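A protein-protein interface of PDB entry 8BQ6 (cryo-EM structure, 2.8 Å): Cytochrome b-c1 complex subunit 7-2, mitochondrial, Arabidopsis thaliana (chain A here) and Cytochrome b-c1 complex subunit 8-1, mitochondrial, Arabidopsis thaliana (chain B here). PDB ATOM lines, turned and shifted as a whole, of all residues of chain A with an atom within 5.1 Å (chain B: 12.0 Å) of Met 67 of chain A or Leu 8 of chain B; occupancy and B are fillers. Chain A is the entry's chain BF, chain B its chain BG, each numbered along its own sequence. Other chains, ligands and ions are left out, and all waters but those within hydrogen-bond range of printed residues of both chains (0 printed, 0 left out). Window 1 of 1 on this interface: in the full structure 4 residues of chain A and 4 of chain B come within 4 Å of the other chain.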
ATOM      1  N   ASN A  63      23.021  32.261  20.459  1.00  0.00           N
ATOM      2  CA  ASN A  63      22.958  31.148  21.401  1.00  0.00           C
ATOM      3  C   ASN A  63      21.604  31.094  22.093  1.00  0.00           C
ATOM      4  O   ASN A  63      21.067  30.009  22.337  1.00  0.00           O
ATOM      5  CB  ASN A  63      24.083  31.249  22.430  1.00  0.00           C
ATOM      6  CG  ASN A  63      25.448  31.013  21.825  1.00  0.00           C
ATOM      7  OD1 ASN A  63      25.590  30.278  20.850  1.00  0.00           O
ATOM      8  ND2 ASN A  63      26.467  31.626  22.412  1.00  0.00           N
ATOM      9  N   GLN A  64      21.037  32.258  22.417  1.00  0.00           N
ATOM     10  CA  GLN A  64      19.739  32.290  23.082  1.00  0.00           C
ATOM     11  C   GLN A  64      18.630  31.780  22.173  1.00  0.00           C
ATOM     12  O   GLN A  64      17.715  31.086  22.631  1.00  0.00           O
ATOM     13  CB  GLN A  64      19.423  33.704  23.551  1.00  0.00           C
ATOM     14  CG  GLN A  64      19.907  33.994  24.941  1.00  0.00           C
ATOM     15  CD  GLN A  64      20.387  35.410  25.085  1.00  0.00           C
ATOM     16  OE1 GLN A  64      20.062  36.272  24.271  1.00  0.00           O
ATOM     17  NE2 GLN A  64      21.175  35.663  26.119  1.00  0.00           N
ATOM     18  N   ARG A  65      18.675  32.140  20.888  1.00  0.00           N
ATOM     19  CA  ARG A  65      17.685  31.625  19.947  1.00  0.00           C
ATOM     20  C   ARG A  65      17.815  30.116  19.796  1.00  0.00           C
ATOM     21  O   ARG A  65      16.815  29.411  19.625  1.00  0.00           O
ATOM     22  CB  ARG A  65      17.837  32.313  18.591  1.00  0.00           C
ATOM     23  CG  ARG A  65      17.257  33.714  18.535  1.00  0.00           C
ATOM     24  CD  ARG A  65      17.194  34.247  17.111  1.00  0.00           C
ATOM     25  NE  ARG A  65      18.501  34.292  16.465  1.00  0.00           N
ATOM     26  CZ  ARG A  65      19.311  35.342  16.475  1.00  0.00           C
ATOM     27  NH1 ARG A  65      18.985  36.462  17.098  1.00  0.00           N
ATOM     28  NH2 ARG A  65      20.478  35.265  15.842  1.00  0.00           N
ATOM     29  N   LEU A  66      19.049  29.608  19.841  1.00  0.00           N
ATOM     30  CA  LEU A  66      19.273  28.168  19.757  1.00  0.00           C
ATOM     31  C   LEU A  66      18.748  27.452  20.993  1.00  0.00           C
ATOM     32  O   LEU A  66      18.184  26.357  20.893  1.00  0.00           O
ATOM     33  CB  LEU A  66      20.759  27.881  19.577  1.00  0.00           C
ATOM     34  CG  LEU A  66      21.342  28.246  18.219  1.00  0.00           C
ATOM     35  CD1 LEU A  66      22.847  28.081  18.245  1.00  0.00           C
ATOM     36  CD2 LEU A  66      20.713  27.400  17.136  1.00  0.00           C
ATOM     37  N   MET A  67      18.957  28.039  22.173  1.00  0.00           N
ATOM     38  CA  MET A  67      18.406  27.455  23.390  1.00  0.00           C
ATOM     39  C   MET A  67      16.885  27.522  23.387  1.00  0.00           C
ATOM     40  O   MET A  67      16.213  26.563  23.785  1.00  0.00           O
ATOM     41  CB  MET A  67      18.980  28.163  24.614  1.00  0.00           C
ATOM     42  CG  MET A  67      18.405  27.691  25.934  1.00  0.00           C
ATOM     43  SD  MET A  67      19.676  27.347  27.162  1.00  0.00           S
ATOM     44  CE  MET A  67      18.664  26.872  28.557  1.00  0.00           C
ATOM     45  N   ARG A  68      16.321  28.644  22.933  1.00  0.00           N
ATOM     46  CA  ARG A  68      14.870  28.748  22.823  1.00  0.00           C
ATOM     47  C   ARG A  68      14.317  27.726  21.837  1.00  0.00           C
ATOM     48  O   ARG A  68      13.309  27.069  22.116  1.00  0.00           O
ATOM     49  CB  ARG A  68      14.476  30.163  22.403  1.00  0.00           C
ATOM     50  CG  ARG A  68      12.982  30.424  22.433  1.00  0.00           C
ATOM     51  CD  ARG A  68      12.669  31.874  22.110  1.00  0.00           C
ATOM     52  NE  ARG A  68      13.106  32.254  20.773  1.00  0.00           N
ATOM     53  CZ  ARG A  68      12.932  33.456  20.244  1.00  0.00           C
ATOM     54  NH1 ARG A  68      12.360  34.435  20.926  1.00  0.00           N
ATOM     55  NH2 ARG A  68      13.342  33.684  19.000  1.00  0.00           N
ATOM     56  N   ALA A  69      14.966  27.580  20.680  1.00  0.00           N
ATOM     57  CA  ALA A  69      14.502  26.616  19.688  1.00  0.00           C
ATOM     58  C   ALA A  69      14.613  25.190  20.208  1.00  0.00           C
ATOM     59  O   ALA A  69      13.724  24.364  19.971  1.00  0.00           O
ATOM     60  CB  ALA A  69      15.290  26.771  18.390  1.00  0.00           C
ATOM     61  N   MET A  70      15.707  24.881  20.908  1.00  0.00           N
ATOM     62  CA  MET A  70      15.873  23.549  21.478  1.00  0.00           C
ATOM     63  C   MET A  70      14.833  23.267  22.546  1.00  0.00           C
ATOM     64  O   MET A  70      14.355  22.135  22.676  1.00  0.00           O
ATOM     65  CB  MET A  70      17.272  23.399  22.061  1.00  0.00           C
ATOM     66  CG  MET A  70      17.871  22.044  21.814  1.00  0.00           C
ATOM     67  SD  MET A  70      19.636  22.144  21.531  1.00  0.00           S
ATOM     68  CE  MET A  70      19.636  22.426  19.776  1.00  0.00           C
ATOM     69  N   ASP A  71      14.497  24.275  23.347  1.00  0.00           N
ATOM     70  CA  ASP A  71      13.472  24.080  24.362  1.00  0.00           C
ATOM     71  C   ASP A  71      12.109  23.836  23.729  1.00  0.00           C
ATOM     72  O   ASP A  71      11.340  22.993  24.202  1.00  0.00           O
ATOM     73  CB  ASP A  71      13.441  25.279  25.305  1.00  0.00           C
ATOM     74  CG  ASP A  71      12.467  25.097  26.438  1.00  0.00           C
ATOM     75  OD1 ASP A  71      11.826  24.029  26.503  1.00  0.00           O
ATOM     76  OD2 ASP A  71      12.359  26.012  27.281  1.00  0.00           O
ATOM     77  N   LEU A  72      11.786  24.568  22.661  1.00  0.00           N
ATOM     78  CA  LEU A  72      10.522  24.328  21.974  1.00  0.00           C
ATOM     79  C   LEU A  72      10.496  22.944  21.343  1.00  0.00           C
ATOM     80  O   LEU A  72       9.508  22.212  21.473  1.00  0.00           O
ATOM     81  CB  LEU A  72      10.288  25.395  20.909  1.00  0.00           C
ATOM     82  CG  LEU A  72       9.985  26.797  21.418  1.00  0.00           C
ATOM     83  CD1 LEU A  72      10.121  27.778  20.277  1.00  0.00           C
ATOM     84  CD2 LEU A  72       8.598  26.849  22.014  1.00  0.00           C
ATOM     85  N   PRO B   5      33.248  25.769  26.765  1.00  0.00           N
ATOM     86  CA  PRO B   5      32.013  26.086  27.487  1.00  0.00           C
ATOM     87  C   PRO B   5      31.378  27.391  27.016  1.00  0.00           C
ATOM     88  O   PRO B   5      32.031  28.434  26.973  1.00  0.00           O
ATOM     89  CB  PRO B   5      32.472  26.190  28.947  1.00  0.00           C
ATOM     90  CG  PRO B   5      33.922  26.469  28.877  1.00  0.00           C
ATOM     91  CD  PRO B   5      34.425  25.779  27.647  1.00  0.00           C
ATOM     92  N   VAL B   6      30.102  27.312  26.665  1.00  0.00           N
ATOM     93  CA  VAL B   6      29.371  28.449  26.123  1.00  0.00           C
ATOM     94  C   VAL B   6      28.840  29.296  27.270  1.00  0.00           C
ATOM     95  O   VAL B   6      28.355  28.772  28.280  1.00  0.00           O
ATOM     96  CB  VAL B   6      28.235  27.956  25.207  1.00  0.00           C
ATOM     97  CG1 VAL B   6      27.385  26.923  25.930  1.00  0.00           C
ATOM     98  CG2 VAL B   6      27.387  29.113  24.712  1.00  0.00           C
ATOM     99  N   LYS B   7      28.951  30.613  27.130  1.00  0.00           N
ATOM    100  CA  LYS B   7      28.445  31.534  28.139  1.00  0.00           C
ATOM    101  C   LYS B   7      26.962  31.775  27.887  1.00  0.00           C
ATOM    102  O   LYS B   7      26.583  32.270  26.821  1.00  0.00           O
ATOM    103  CB  LYS B   7      29.222  32.846  28.096  1.00  0.00           C
ATOM    104  CG  LYS B   7      30.729  32.678  28.036  1.00  0.00           C
ATOM    105  CD  LYS B   7      31.238  31.792  29.152  1.00  0.00           C
ATOM    106  CE  LYS B   7      32.166  32.573  30.069  1.00  0.00           C
ATOM    107  NZ  LYS B   7      33.242  31.719  30.634  1.00  0.00           N
ATOM    108  N   LEU B   8      26.125  31.430  28.863  1.00  0.00           N
ATOM    109  CA  LEU B   8      24.679  31.437  28.696  1.00  0.00           C
ATOM    110  C   LEU B   8      24.040  32.232  29.826  1.00  0.00           C
ATOM    111  O   LEU B   8      24.364  32.032  31.001  1.00  0.00           O
ATOM    112  CB  LEU B   8      24.148  29.985  28.646  1.00  0.00           C
ATOM    113  CG  LEU B   8      22.675  29.588  28.463  1.00  0.00           C
ATOM    114  CD1 LEU B   8      21.848  29.587  29.741  1.00  0.00           C
ATOM    115  CD2 LEU B   8      22.046  30.502  27.426  1.00  0.00           C
ATOM    116  N   LYS B   9      23.152  33.155  29.470  1.00  0.00           N
ATOM    117  CA  LYS B   9      22.386  33.930  30.437  1.00  0.00           C
ATOM    118  C   LYS B   9      20.917  33.565  30.292  1.00  0.00           C
ATOM    119  O   LYS B   9      20.321  33.796  29.234  1.00  0.00           O
ATOM    120  CB  LYS B   9      22.599  35.433  30.239  1.00  0.00           C
ATOM    121  CG  LYS B   9      21.831  36.290  31.222  1.00  0.00           C
ATOM    122  CD  LYS B   9      22.719  36.783  32.340  1.00  0.00           C
ATOM    123  CE  LYS B   9      22.049  37.900  33.115  1.00  0.00           C
ATOM    124  NZ  LYS B   9      22.670  39.220  32.830  1.00  0.00           N
ATOM    125  N   ALA B  10      20.338  32.990  31.345  1.00  0.00           N
ATOM    126  CA  ALA B  10      18.957  32.533  31.303  1.00  0.00           C
ATOM    127  C   ALA B  10      18.456  32.310  32.721  1.00  0.00           C
ATOM    128  O   ALA B  10      19.241  32.166  33.660  1.00  0.00           O
ATOM    129  CB  ALA B  10      18.815  31.244  30.491  1.00  0.00           C
ATOM    130  N   VAL B  11      17.134  32.277  32.860  1.00  0.00           N
ATOM    131  CA  VAL B  11      16.477  31.918  34.110  1.00  0.00           C
ATOM    132  C   VAL B  11      15.543  30.751  33.829  1.00  0.00           C
ATOM    133  O   VAL B  11      14.732  30.809  32.899  1.00  0.00           O
ATOM    134  CB  VAL B  11      15.705  33.102  34.716  1.00  0.00           C
ATOM    135  CG1 VAL B  11      15.054  32.688  36.027  1.00  0.00           C
ATOM    136  CG2 VAL B  11      16.627  34.283  34.922  1.00  0.00           C
ATOM    137  N   VAL B  12      15.666  29.692  34.625  1.00  0.00           N
ATOM    138  CA  VAL B  12      14.875  28.480  34.456  1.00  0.00           C
ATOM    139  C   VAL B  12      14.131  28.209  35.752  1.00  0.00           C
ATOM    140  O   VAL B  12      14.747  28.113  36.820  1.00  0.00           O
ATOM    141  CB  VAL B  12      15.746  27.272  34.077  1.00  0.00           C
ATOM    142  CG1 VAL B  12      14.872  26.105  33.661  1.00  0.00           C
ATOM    143  CG2 VAL B  12      16.713  27.635  32.973  1.00  0.00           C
ATOM    144  N   TYR B  13      12.814  28.076  35.656  1.00  0.00           N
ATOM    145  CA  TYR B  13      11.982  27.618  36.759  1.00  0.00           C
ATOM    146  C   TYR B  13      11.497  26.212  36.444  1.00  0.00           C
ATOM    147  O   TYR B  13      11.000  25.957  35.344  1.00  0.00           O
ATOM    148  CB  TYR B  13      10.780  28.537  36.981  1.00  0.00           C
ATOM    149  CG  TYR B  13      11.077  30.015  36.960  1.00  0.00           C
ATOM    150  CD1 TYR B  13      11.227  30.695  35.761  1.00  0.00           C
ATOM    151  CD2 TYR B  13      11.171  30.738  38.137  1.00  0.00           C
ATOM    152  CE1 TYR B  13      11.487  32.039  35.737  1.00  0.00           C
ATOM    153  CE2 TYR B  13      11.427  32.090  38.121  1.00  0.00           C
ATOM    154  CZ  TYR B  13      11.583  32.735  36.917  1.00  0.00           C
ATOM    155  OH  TYR B  13      11.841  34.082  36.887  1.00  0.00           O
ATOM    156  N   ALA B  14      11.632  25.306  37.408  1.00  0.00           N
ATOM    157  CA  ALA B  14      11.226  23.923  37.227  1.00  0.00           C
ATOM    158  C   ALA B  14      10.376  23.475  38.405  1.00  0.00           C
ATOM    159  O   ALA B  14      10.512  23.983  39.520  1.00  0.00           O
ATOM    160  CB  ALA B  14      12.439  23.000  37.072  1.00  0.00           C
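Of chain B, only Leu 8 comes within 4 Å of Met 67 of chain A.
Asn 63 of chain A touches one residue of chain B.
No residue of chain B comes within 4 Å of Leu 66 of chain A.
No residue of chain B comes within 4 Å of Ala 69 of chain A.
Met 70 of chain A touches none of the printed residues of chain B.
Of the printed residues of chain A, Val 6 of chain B touches Asn 63.
Printed residues of chain A within 4 Å of Lys 9 of chain B: Gln 64.
Leu 72 of chain A touches none of the printed residues of chain B.
Lys 7 of chain B touches none of the printed residues of chain A.
The nearest residue of chain B that does not touch Met 67 of chain A is Ala 10 of chain B (4.8 Å).
Among the printed residues, merely in contact across the chains: Asn 63 of chain A with Val 6 of chain B, Gln 64 of chain A with Lys 9 of chain B and Met 67 of chain A with Leu 8 of chain B.
Of the 10 printed residues of chain A, 3 touch a printed residue of chain B.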
